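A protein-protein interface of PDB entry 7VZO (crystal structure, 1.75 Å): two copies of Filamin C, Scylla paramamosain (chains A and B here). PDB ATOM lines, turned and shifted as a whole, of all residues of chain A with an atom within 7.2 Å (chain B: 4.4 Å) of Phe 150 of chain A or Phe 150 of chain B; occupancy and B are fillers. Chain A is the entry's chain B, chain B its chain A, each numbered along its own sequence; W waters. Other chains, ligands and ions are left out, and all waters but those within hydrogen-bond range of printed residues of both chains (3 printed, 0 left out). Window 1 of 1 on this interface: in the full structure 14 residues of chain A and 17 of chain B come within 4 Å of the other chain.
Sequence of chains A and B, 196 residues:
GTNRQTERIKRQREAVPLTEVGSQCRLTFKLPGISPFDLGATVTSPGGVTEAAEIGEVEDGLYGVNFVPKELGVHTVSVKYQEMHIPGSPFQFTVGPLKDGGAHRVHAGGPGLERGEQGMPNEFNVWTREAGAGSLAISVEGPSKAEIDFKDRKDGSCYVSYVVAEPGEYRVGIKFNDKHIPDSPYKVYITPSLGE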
ATOM      1  N   ILE A   9     -20.709  29.083  28.026  1.00  0.00           N
ATOM      2  CA  ILE A   9     -20.608  27.634  27.792  1.00  0.00           C
ATOM      3  C   ILE A   9     -19.187  27.353  27.343  1.00  0.00           C
ATOM      4  O   ILE A   9     -18.465  28.297  26.886  1.00  0.00           O
ATOM      5  CB  ILE A   9     -21.662  27.173  26.767  1.00  0.00           C
ATOM      6  CG1 ILE A   9     -21.593  27.853  25.405  1.00  0.00           C
ATOM      7  CG2 ILE A   9     -23.051  27.367  27.376  1.00  0.00           C
ATOM      8  CD1 ILE A   9     -20.547  27.262  24.482  1.00  0.00           C
ATOM      9  N   LYS A  10     -18.794  26.105  27.468  1.00  0.00           N
ATOM     10  CA  LYS A  10     -17.475  25.685  26.967  1.00  0.00           C
ATOM     11  C   LYS A  10     -17.619  24.324  26.328  1.00  0.00           C
ATOM     12  O   LYS A  10     -18.411  23.536  26.801  1.00  0.00           O
ATOM     13  CB  LYS A  10     -16.423  25.572  28.076  1.00  0.00           C
ATOM     14  CG  LYS A  10     -16.135  26.836  28.821  1.00  0.00           C
ATOM     15  CD  LYS A  10     -14.912  26.648  29.732  1.00  0.00           C
ATOM     16  CE  LYS A  10     -14.841  27.718  30.786  1.00  0.00           C
ATOM     17  NZ  LYS A  10     -13.489  27.785  31.393  1.00  0.00           N
ATOM     18  N   ARG A  11     -16.748  24.020  25.381  1.00  0.00           N
ATOM     19  CA  ARG A  11     -16.637  22.657  24.875  1.00  0.00           C
ATOM     20  C   ARG A  11     -15.157  22.328  24.734  1.00  0.00           C
ATOM     21  O   ARG A  11     -14.361  23.256  24.473  1.00  0.00           O
ATOM     22  CB  ARG A  11     -17.416  22.484  23.569  1.00  0.00           C
ATOM     23  CG  ARG A  11     -16.754  23.099  22.367  1.00  0.00           C
ATOM     24  CD  ARG A  11     -15.704  22.203  21.751  1.00  0.00           C
ATOM     25  NE  ARG A  11     -15.237  22.676  20.440  1.00  0.00           N
ATOM     26  CZ  ARG A  11     -13.972  22.894  20.079  1.00  0.00           C
ATOM     27  NH1 ARG A  11     -12.973  22.860  20.957  1.00  0.00           N
ATOM     28  NH2 ARG A  11     -13.714  23.099  18.795  1.00  0.00           N
ATOM     29  N   GLN A  12     -14.816  21.059  24.894  1.00  0.00           N
ATOM     30  CA  GLN A  12     -13.471  20.549  24.640  1.00  0.00           C
ATOM     31  C   GLN A  12     -13.551  19.473  23.573  1.00  0.00           C
ATOM     32  O   GLN A  12     -14.467  18.625  23.619  1.00  0.00           O
ATOM     33  CB  GLN A  12     -12.873  19.988  25.922  1.00  0.00           C
ATOM     34  CG  GLN A  12     -12.506  21.073  26.888  1.00  0.00           C
ATOM     35  CD  GLN A  12     -13.611  21.267  27.878  1.00  0.00           C
ATOM     36  OE1 GLN A  12     -14.148  20.297  28.443  1.00  0.00           O
ATOM     37  NE2 GLN A  12     -13.923  22.524  28.133  1.00  0.00           N
ATOM     38  N   ARG A  13     -12.597  19.493  22.675  1.00  0.00           N
ATOM     39  CA  ARG A  13     -12.561  18.542  21.550  1.00  0.00           C
ATOM     40  C   ARG A  13     -11.091  18.313  21.214  1.00  0.00           C
ATOM     41  O   ARG A  13     -10.276  19.217  21.410  1.00  0.00           O
ATOM     42  CB  ARG A  13     -13.364  19.148  20.384  1.00  0.00           C
ATOM     43  CG  ARG A  13     -13.355  18.292  19.133  1.00  0.00           C
ATOM     44  CD  ARG A  13     -14.175  18.914  18.018  1.00  0.00           C
ATOM     45  NE  ARG A  13     -15.619  18.863  18.208  1.00  0.00           N
ATOM     46  CZ  ARG A  13     -16.386  17.839  17.828  1.00  0.00           C
ATOM     47  NH1 ARG A  13     -15.878  16.716  17.343  1.00  0.00           N
ATOM     48  NH2 ARG A  13     -17.685  17.947  17.924  1.00  0.00           N
ATOM     49  N   LEU A 136     -13.009  25.627  23.783  1.00  0.00           N
ATOM     50  CA  LEU A 136     -13.625  26.836  23.201  1.00  0.00           C
ATOM     51  C   LEU A 136     -14.668  27.330  24.203  1.00  0.00           C
ATOM     52  O   LEU A 136     -15.524  26.526  24.607  1.00  0.00           O
ATOM     53  CB  LEU A 136     -14.248  26.489  21.859  1.00  0.00           C
ATOM     54  CG  LEU A 136     -14.947  27.635  21.149  1.00  0.00           C
ATOM     55  CD1 LEU A 136     -13.960  28.707  20.749  1.00  0.00           C
ATOM     56  CD2 LEU A 136     -15.757  27.128  19.945  1.00  0.00           C
ATOM     57  N   ILE A 138     -17.486  30.344  25.064  1.00  0.00           N
ATOM     58  CA  ILE A 138     -18.355  31.399  24.492  1.00  0.00           C
ATOM     59  C   ILE A 138     -19.072  32.076  25.653  1.00  0.00           C
ATOM     60  O   ILE A 138     -19.720  31.379  26.433  1.00  0.00           O
ATOM     61  CB  ILE A 138     -19.390  30.832  23.516  1.00  0.00           C
ATOM     62  CG1 ILE A 138     -18.819  29.923  22.420  1.00  0.00           C
ATOM     63  CG2 ILE A 138     -20.152  31.989  22.923  1.00  0.00           C
ATOM     64  CD1 ILE A 138     -17.917  30.637  21.495  1.00  0.00           C
ATOM     65  N   ILE A 148     -28.179  30.261  25.536  1.00  0.00           N
ATOM     66  CA  ILE A 148     -27.168  29.932  24.494  1.00  0.00           C
ATOM     67  C   ILE A 148     -27.353  28.475  24.086  1.00  0.00           C
ATOM     68  O   ILE A 148     -27.276  27.598  24.959  1.00  0.00           O
ATOM     69  CB  ILE A 148     -25.723  30.169  24.988  1.00  0.00           C
ATOM     70  CG1 ILE A 148     -25.422  31.611  25.426  1.00  0.00           C
ATOM     71  CG2 ILE A 148     -24.764  29.701  23.907  1.00  0.00           C
ATOM     72  CD1 ILE A 148     -24.051  31.771  26.025  1.00  0.00           C
ATOM     73  N   ASP A 149     -27.494  28.239  22.792  1.00  0.00           N
ATOM     74  CA  ASP A 149     -27.455  26.892  22.173  1.00  0.00           C
ATOM     75  C   ASP A 149     -26.228  26.828  21.275  1.00  0.00           C
ATOM     76  O   ASP A 149     -25.825  27.860  20.703  1.00  0.00           O
ATOM     77  CB  ASP A 149     -28.662  26.593  21.295  1.00  0.00           C
ATOM     78  CG  ASP A 149     -29.992  26.472  22.000  1.00  0.00           C
ATOM     79  OD1 ASP A 149     -30.009  26.424  23.241  1.00  0.00           O
ATOM     80  OD2 ASP A 149     -31.019  26.435  21.261  1.00  0.00           O
ATOM     81  N   PHE A 150     -25.663  25.652  21.098  1.00  0.00           N
ATOM     82  CA  PHE A 150     -24.576  25.547  20.101  1.00  0.00           C
ATOM     83  C   PHE A 150     -24.542  24.169  19.489  1.00  0.00           C
ATOM     84  O   PHE A 150     -24.874  23.160  20.161  1.00  0.00           O
ATOM     85  CB  PHE A 150     -23.233  25.982  20.691  1.00  0.00           C
ATOM     86  CG  PHE A 150     -22.662  25.090  21.770  1.00  0.00           C
ATOM     87  CD1 PHE A 150     -23.070  25.241  23.067  1.00  0.00           C
ATOM     88  CD2 PHE A 150     -21.768  24.098  21.463  1.00  0.00           C
ATOM     89  CE1 PHE A 150     -22.571  24.410  24.067  1.00  0.00           C
ATOM     90  CE2 PHE A 150     -21.245  23.284  22.466  1.00  0.00           C
ATOM     91  CZ  PHE A 150     -21.650  23.463  23.766  1.00  0.00           C
ATOM     92  N   LYS A 151     -24.066  24.140  18.265  1.00  0.00           N
ATOM     93  CA  LYS A 151     -23.792  22.865  17.577  1.00  0.00           C
ATOM     94  C   LYS A 151     -22.288  22.813  17.281  1.00  0.00           C
ATOM     95  O   LYS A 151     -21.786  23.612  16.443  1.00  0.00           O
ATOM     96  CB  LYS A 151     -24.672  22.684  16.334  1.00  0.00           C
ATOM     97  CG  LYS A 151     -24.419  21.319  15.714  1.00  0.00           C
ATOM     98  CD  LYS A 151     -25.378  20.830  14.685  1.00  0.00           C
ATOM     99  CE  LYS A 151     -24.954  19.478  14.135  1.00  0.00           C
ATOM    100  NZ  LYS A 151     -26.031  18.868  13.309  1.00  0.00           N
ATOM    101  N   ASP A 152     -21.637  21.812  17.835  1.00  0.00           N
ATOM    102  CA  ASP A 152     -20.188  21.611  17.713  1.00  0.00           C
ATOM    103  C   ASP A 152     -19.917  20.442  16.789  1.00  0.00           C
ATOM    104  O   ASP A 152     -20.435  19.340  17.040  1.00  0.00           O
ATOM    105  CB  ASP A 152     -19.584  21.502  19.107  1.00  0.00           C
ATOM    106  CG  ASP A 152     -18.080  21.508  19.063  1.00  0.00           C
ATOM    107  OD1 ASP A 152     -17.494  22.619  18.789  1.00  0.00           O
ATOM    108  OD2 ASP A 152     -17.496  20.470  19.402  1.00  0.00           O
ATOM    109  N   ARG A 153     -19.166  20.666  15.713  1.00  0.00           N
ATOM    110  CA  ARG A 153     -19.037  19.679  14.623  1.00  0.00           C
ATOM    111  C   ARG A 153     -17.639  19.087  14.550  1.00  0.00           C
ATOM    112  O   ARG A 153     -16.648  19.715  14.962  1.00  0.00           O
ATOM    113  CB  ARG A 153     -19.373  20.330  13.272  1.00  0.00           C
ATOM    114  CG  ARG A 153     -20.808  20.775  13.126  1.00  0.00           C
ATOM    115  CD  ARG A 153     -21.072  21.551  11.841  1.00  0.00           C
ATOM    116  NE  ARG A 153     -22.526  21.555  11.563  1.00  0.00           N
ATOM    117  CZ  ARG A 153     -23.414  22.450  12.006  1.00  0.00           C
ATOM    118  NH1 ARG A 153     -23.041  23.457  12.794  1.00  0.00           N
ATOM    119  NH2 ARG A 153     -24.688  22.331  11.657  1.00  0.00           N
ATOM    120  N   LYS A 154     -17.589  17.916  13.911  1.00  0.00           N
ATOM    121  CA  LYS A 154     -16.361  17.126  13.705  1.00  0.00           C
ATOM    122  C   LYS A 154     -15.334  17.921  12.908  1.00  0.00           C
ATOM    123  O   LYS A 154     -14.169  17.544  12.980  1.00  0.00           O
ATOM    124  CB  LYS A 154     -16.704  15.826  12.973  1.00  0.00           C
ATOM    125  CG  LYS A 154     -17.386  16.094  11.639  1.00  0.00           C
ATOM    126  CD  LYS A 154     -17.463  14.915  10.724  1.00  0.00           C
ATOM    127  CE  LYS A 154     -18.517  15.110   9.652  1.00  0.00           C
ATOM    128  NZ  LYS A 154     -18.386  14.054   8.630  1.00  0.00           N
ATOM    129  N   CYS A 158     -18.121  25.470  15.247  1.00  0.00           N
ATOM    130  CA  CYS A 158     -19.142  25.521  16.313  1.00  0.00           C
ATOM    131  C   CYS A 158     -20.069  26.666  15.956  1.00  0.00           C
ATOM    132  O   CYS A 158     -19.568  27.843  15.835  1.00  0.00           O
ATOM    133  CB  CYS A 158     -18.451  25.757  17.645  1.00  0.00           C
ATOM    134  SG  CYS A 158     -19.573  25.738  19.064  1.00  0.00           S
ATOM    135  N   TYR A 159     -21.347  26.365  15.801  1.00  0.00           N
ATOM    136  CA  TYR A 159     -22.365  27.339  15.372  1.00  0.00           C
ATOM    137  C   TYR A 159     -23.184  27.685  16.604  1.00  0.00           C
ATOM    138  O   TYR A 159     -23.671  26.754  17.272  1.00  0.00           O
ATOM    139  CB  TYR A 159     -23.219  26.770  14.257  1.00  0.00           C
ATOM    140  CG  TYR A 159     -24.003  27.819  13.540  1.00  0.00           C
ATOM    141  CD1 TYR A 159     -25.230  28.237  14.017  1.00  0.00           C
ATOM    142  CD2 TYR A 159     -23.472  28.433  12.421  1.00  0.00           C
ATOM    143  CE1 TYR A 159     -25.962  29.199  13.345  1.00  0.00           C
ATOM    144  CE2 TYR A 159     -24.183  29.416  11.752  1.00  0.00           C
ATOM    145  CZ  TYR A 159     -25.434  29.804  12.217  1.00  0.00           C
ATOM    146  OH  TYR A 159     -26.174  30.767  11.576  1.00  0.00           O
ATOM    147  N   VAL A 160     -23.238  28.963  16.927  1.00  0.00           N
ATOM    148  CA  VAL A 160     -23.866  29.442  18.171  1.00  0.00           C
ATOM    149  C   VAL A 160     -25.122  30.231  17.842  1.00  0.00           C
ATOM    150  O   VAL A 160     -25.094  31.056  16.904  1.00  0.00           O
ATOM    151  CB  VAL A 160     -22.849  30.289  18.957  1.00  0.00           C
ATOM    152  CG1 VAL A 160     -23.489  30.788  20.214  1.00  0.00           C
ATOM    153  CG2 VAL A 160     -21.558  29.556  19.251  1.00  0.00           C
ATOM    154  N   SER A 161     -26.136  30.085  18.690  1.00  0.00           N
ATOM    155  CA  SER A 161     -27.372  30.877  18.660  1.00  0.00           C
ATOM    156  C   SER A 161     -27.629  31.312  20.108  1.00  0.00           C
ATOM    157  O   SER A 161     -27.745  30.429  20.973  1.00  0.00           O
ATOM    158  CB  SER A 161     -28.509  30.122  18.073  1.00  0.00           C
ATOM    159  OG  SER A 161     -29.707  30.893  17.978  1.00  0.00           O
ATOM    160  N   ILE B   9     -15.603  14.056  23.539  1.00  0.00           N
ATOM    161  CA  ILE B   9     -15.945  15.490  23.581  1.00  0.00           C
ATOM    162  C   ILE B   9     -16.455  15.770  24.999  1.00  0.00           C
ATOM    163  O   ILE B   9     -16.877  14.831  25.742  1.00  0.00           O
ATOM    164  CB  ILE B   9     -16.987  15.885  22.527  1.00  0.00           C
ATOM    165  CG1 ILE B   9     -18.287  15.116  22.706  1.00  0.00           C
ATOM    166  CG2 ILE B   9     -16.410  15.690  21.125  1.00  0.00           C
ATOM    167  CD1 ILE B   9     -19.312  15.805  23.584  1.00  0.00           C
ATOM    168  N   LYS B  10     -16.450  17.027  25.361  1.00  0.00           N
ATOM    169  CA  LYS B  10     -17.058  17.440  26.658  1.00  0.00           C
ATOM    170  C   LYS B  10     -17.692  18.804  26.457  1.00  0.00           C
ATOM    171  O   LYS B  10     -17.167  19.595  25.643  1.00  0.00           O
ATOM    172  CB  LYS B  10     -16.038  17.571  27.793  1.00  0.00           C
ATOM    173  CG  LYS B  10     -15.132  16.384  28.032  1.00  0.00           C
ATOM    174  CD  LYS B  10     -14.499  16.455  29.459  1.00  0.00           C
ATOM    175  CE  LYS B  10     -13.206  15.673  29.576  1.00  0.00           C
ATOM    176  NZ  LYS B  10     -13.449  14.239  29.814  1.00  0.00           N
ATOM    177  N   ARG B  11     -18.663  19.128  27.279  1.00  0.00           N
ATOM    178  CA  ARG B  11     -19.156  20.508  27.374  1.00  0.00           C
ATOM    179  C   ARG B  11     -19.409  20.847  28.844  1.00  0.00           C
ATOM    180  O   ARG B  11     -19.813  19.951  29.628  1.00  0.00           O
ATOM    181  CB  ARG B  11     -20.392  20.640  26.492  1.00  0.00           C
ATOM    182  CG  ARG B  11     -21.650  19.980  27.023  1.00  0.00           C
ATOM    183  CD  ARG B  11     -22.391  20.885  27.971  1.00  0.00           C
ATOM    184  NE  ARG B  11     -23.739  20.441  28.354  1.00  0.00           N
ATOM    185  CZ  ARG B  11     -24.164  20.178  29.583  1.00  0.00           C
ATOM    186  NH1 ARG B  11     -23.362  20.202  30.638  1.00  0.00           N
ATOM    187  NH2 ARG B  11     -25.433  19.918  29.750  1.00  0.00           N
ATOM    188  N   ARG B  13     -21.675  23.623  31.232  1.00  0.00           N
ATOM    189  CA  ARG B  13     -22.832  24.528  31.274  1.00  0.00           C
ATOM    190  C   ARG B  13     -23.274  24.676  32.733  1.00  0.00           C
ATOM    191  O   ARG B  13     -23.209  23.703  33.479  1.00  0.00           O
ATOM    192  CB  ARG B  13     -23.941  23.946  30.384  1.00  0.00           C
ATOM    193  CG  ARG B  13     -25.128  24.850  30.172  1.00  0.00           C
ATOM    194  CD  ARG B  13     -26.184  24.206  29.315  1.00  0.00           C
ATOM    195  NE  ARG B  13     -25.899  24.232  27.894  1.00  0.00           N
ATOM    196  CZ  ARG B  13     -26.203  25.265  27.100  1.00  0.00           C
ATOM    197  NH1 ARG B  13     -26.730  26.390  27.587  1.00  0.00           N
ATOM    198  NH2 ARG B  13     -26.050  25.133  25.798  1.00  0.00           N
ATOM    199  N   ASP B 149     -20.575  14.776  16.320  1.00  0.00           N
ATOM    200  CA  ASP B 149     -21.185  16.125  16.318  1.00  0.00           C
ATOM    201  C   ASP B 149     -22.161  16.184  17.490  1.00  0.00           C
ATOM    202  O   ASP B 149     -22.754  15.167  17.823  1.00  0.00           O
ATOM    203  CB  ASP B 149     -22.013  16.403  15.074  1.00  0.00           C
ATOM    204  CG  ASP B 149     -21.256  16.592  13.773  1.00  0.00           C
ATOM    205  OD1 ASP B 149     -20.008  16.654  13.806  1.00  0.00           O
ATOM    206  OD2 ASP B 149     -21.947  16.602  12.705  1.00  0.00           O
ATOM    207  N   PHE B 150     -22.386  17.347  18.055  1.00  0.00           N
ATOM    208  CA  PHE B 150     -23.399  17.434  19.116  1.00  0.00           C
ATOM    209  C   PHE B 150     -24.050  18.798  19.125  1.00  0.00           C
ATOM    210  O   PHE B 150     -23.417  19.797  18.800  1.00  0.00           O
ATOM    211  CB  PHE B 150     -22.823  16.984  20.458  1.00  0.00           C
ATOM    212  CG  PHE B 150     -21.833  17.902  21.081  1.00  0.00           C
ATOM    213  CD1 PHE B 150     -20.490  17.761  20.789  1.00  0.00           C
ATOM    214  CD2 PHE B 150     -22.233  18.874  21.990  1.00  0.00           C
ATOM    215  CE1 PHE B 150     -19.554  18.601  21.375  1.00  0.00           C
ATOM    216  CE2 PHE B 150     -21.284  19.687  22.606  1.00  0.00           C
ATOM    217  CZ  PHE B 150     -19.953  19.527  22.299  1.00  0.00           C
ATOM    218  N   LYS B 151     -25.316  18.829  19.539  1.00  0.00           N
ATOM    219  CA  LYS B 151     -26.052  20.097  19.698  1.00  0.00           C
ATOM    220  C   LYS B 151     -26.478  20.198  21.161  1.00  0.00           C
ATOM    221  O   LYS B 151     -27.212  19.321  21.630  1.00  0.00           O
ATOM    222  CB  LYS B 151     -27.255  20.244  18.776  1.00  0.00           C
ATOM    223  CG  LYS B 151     -27.858  21.637  18.922  1.00  0.00           C
ATOM    224  CD  LYS B 151     -28.820  22.025  17.870  1.00  0.00           C
ATOM    225  CE  LYS B 151     -29.534  23.292  18.233  1.00  0.00           C
ATOM    226  NZ  LYS B 151     -30.325  23.785  17.081  1.00  0.00           N
ATOM    227  N   ASP B 152     -25.994  21.213  21.844  1.00  0.00           N
ATOM    228  CA  ASP B 152     -26.184  21.384  23.300  1.00  0.00           C
ATOM    229  C   ASP B 152     -27.114  22.571  23.507  1.00  0.00           C
ATOM    230  O   ASP B 152     -26.795  23.654  23.001  1.00  0.00           O
ATOM    231  CB  ASP B 152     -24.822  21.511  23.949  1.00  0.00           C
ATOM    232  CG  ASP B 152     -24.950  21.525  25.452  1.00  0.00           C
ATOM    233  OD1 ASP B 152     -25.256  20.433  26.034  1.00  0.00           O
ATOM    234  OD2 ASP B 152     -24.847  22.631  26.017  1.00  0.00           O
ATOM    235  N   CYS B 158     -28.862  17.562  25.169  1.00  0.00           N
ATOM    236  CA  CYS B 158     -27.738  17.467  24.212  1.00  0.00           C
ATOM    237  C   CYS B 158     -28.035  16.328  23.255  1.00  0.00           C
ATOM    238  O   CYS B 158     -28.166  15.185  23.725  1.00  0.00           O
ATOM    239  CB  CYS B 158     -26.452  17.208  24.985  1.00  0.00           C
ATOM    240  SG  CYS B 158     -24.926  17.311  24.007  1.00  0.00           S
ATOM    241  N   TYR B 159     -28.025  16.577  21.954  1.00  0.00           N
ATOM    242  CA  TYR B 159     -28.300  15.566  20.938  1.00  0.00           C
ATOM    243  C   TYR B 159     -26.993  15.284  20.228  1.00  0.00           C
ATOM    244  O   TYR B 159     -26.318  16.247  19.816  1.00  0.00           O
ATOM    245  CB  TYR B 159     -29.352  16.045  19.962  1.00  0.00           C
ATOM    246  CG  TYR B 159     -29.940  14.907  19.187  1.00  0.00           C
ATOM    247  CD1 TYR B 159     -30.941  14.126  19.741  1.00  0.00           C
ATOM    248  CD2 TYR B 159     -29.565  14.657  17.889  1.00  0.00           C
ATOM    249  CE1 TYR B 159     -31.495  13.065  19.026  1.00  0.00           C
ATOM    250  CE2 TYR B 159     -30.146  13.644  17.143  1.00  0.00           C
ATOM    251  CZ  TYR B 159     -31.112  12.835  17.716  1.00  0.00           C
ATOM    252  OH  TYR B 159     -31.734  11.818  17.023  1.00  0.00           O
ATOM    253  N   VAL B 160     -26.626  14.012  20.174  1.00  0.00           N
ATOM    254  CA  VAL B 160     -25.325  13.521  19.672  1.00  0.00           C
ATOM    255  C   VAL B 160     -25.574  12.710  18.400  1.00  0.00           C
ATOM    256  O   VAL B 160     -26.463  11.835  18.391  1.00  0.00           O
ATOM    257  CB  VAL B 160     -24.625  12.658  20.733  1.00  0.00           C
ATOM    258  CG1 VAL B 160     -23.267  12.165  20.253  1.00  0.00           C
ATOM    259  CG2 VAL B 160     -24.463  13.413  22.055  1.00  0.00           C
HETATM  260  O   HOH W   1     -24.560  16.247  12.641  1.00  0.00           O
HETATM  261  O   HOH W   2     -31.050  26.681  18.582  1.00  0.00           O
HETATM  262  O   HOH W   3     -27.984  29.105  28.193  1.00  0.00           O
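The side-chain carboxylate (OD1) of Asp 152 of chain B is in salt-bridge range of the guanidinium group (NE) of Arg 11 of chain B (2.8 Å). OD2 of Asp 152 of chain B lies within salt-bridge range of NE of Arg 13 of chain B. N of Lys 151 of chain A sits at hydrogen-bond distance from O of Tyr 159 of chain A (2.8 Å). O of Ile 9 of chain A is in hydrogen-bond range of N of Ile 138 of chain A (2.9 Å). SG of Cys 158 of chain B lies close to OD1 of Asp 152 of chain B, 3.7 Å away. The backbone carbonyl oxygen of Ser 161 of chain A is in hydrogen-bond range of the backbone NH of Asp 149 of chain A.
Water W1 lies within hydrogen-bond range of the side-chain carboxylate (OD2) of Asp 149 of chain B (2.6 Å) and the side-chain amino group (NZ) of Lys 151 of chain A (3.1 Å). Water W2 bridges OD2 of Asp 149 of chain A and NZ of Lys 151 of chain B. Water W3 lies within hydrogen-bond range of N of Ile 148 of chain A (2.9 Å) and NH1 of Arg 13 of chain B (3.1 Å).
Arg 13 of chain A touches Phe 150 of chain B, and with the chains exchanged Phe 150 of chain A touches Arg 13 of chain B. Asp 149 of chain A touches Asp 152 of chain B, and with the chains exchanged Asp 152 of chain A touches Asp 149 of chain B. Phe 150 of chain A touches its own counterpart, Phe 150 of chain B. Phe 150 of chain A touches Asp 152 of chain B, and with the chains exchanged Asp 152 of chain A touches Phe 150 of chain B. Of the 18 pairs that touch across the chains among the printed residues, 13 have their exchanged pair printed and touching as well.
Printed residues of chain B within 4 Å of Ile 9 of chain A: Arg 13 (3.8 Å). Leu 136 of chain A touches none of the printed residues of chain B. Of the printed residues of chain B, Asp 149 of chain A touches Asp 152. Phe 150 of chain A touches four residues of chain B. Of the printed residues of chain A, Ile 9 of chain B touches Gln 12 and Arg 13. Phe 150 of chain B touches just these residues of chain A: Arg 13, Phe 150, Lys 151 and Asp 152. Val 160 of chain B touches none of the printed residues of chain A. The nearest residue of chain B that does not touch Phe 150 of chain A is Arg 11 of chain B (4.1 Å).
Among the printed residues, pairs that only touch across the chains: Lys 10 of chain A with Arg 11 of chain B (3.2 Å), Arg 11 of chain A with Lys 10 of chain B (3.2 Å), Arg 153 of chain A with Asp 149 of chain B (3.3 Å), Phe 150 of chain A with Lys 151 of chain B (3.3 Å), Lys 151 of chain A with Phe 150 of chain B (3.3 Å), Asp 152 of chain A with Asp 149 of chain B (3.4 Å), Asp 149 of chain A with Asp 152 of chain B (3.4 Å), Gln 12 of chain A with Ile 9 of chain B (3.5 Å), Phe 150 of chain A with Phe 150 of chain B (3.6 Å), Ile 9 of chain A with Arg 13 of chain B (3.8 Å), Arg 13 of chain A with Ile 9 of chain B (3.9 Å), Phe 150 of chain A with Arg 13 of chain B (3.95 Å) and Arg 13 of chain A with Phe 150 of chain B (3.98 Å).
The backbone NH (N) of Gln 12 of chain A sits at hydrogen-bond distance from the backbone carbonyl oxygen (O) of Lys 10 of chain B (2.9 Å). O of Phe 150 of chain B lies within hydrogen-bond range of N of Asp 152 of chain A, at 2.9 Å. N of Asp 152 of chain B sits at hydrogen-bond distance from O of Phe 150 of chain A (2.8 Å). The side-chain carboxylate (OD1) of Asp 149 of chain B lies within hydrogen-bond range of the backbone NH (N) of Lys 154 of chain A. The guanidinium group of Arg 13 of chain B is in hydrogen-bond range of the backbone carbonyl oxygen of Ile 148 of chain A.
Printed residues of chain A that touch a printed residue of chain B: Ile 9, Lys 10, Arg 11, Gln 12, Arg 13, Ile 148, Asp 149, Phe 150, Lys 151, Asp 152, Arg 153 and Lys 154. Hydrophobic or aromatic side chains of chain B within 4 Å of the printed part of chain A: Ile 9 and Phe 150. Among the printed residues, no Asp or Glu carboxylate lies within 4 Å of a Lys or Arg side-chain nitrogen of the other chain.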
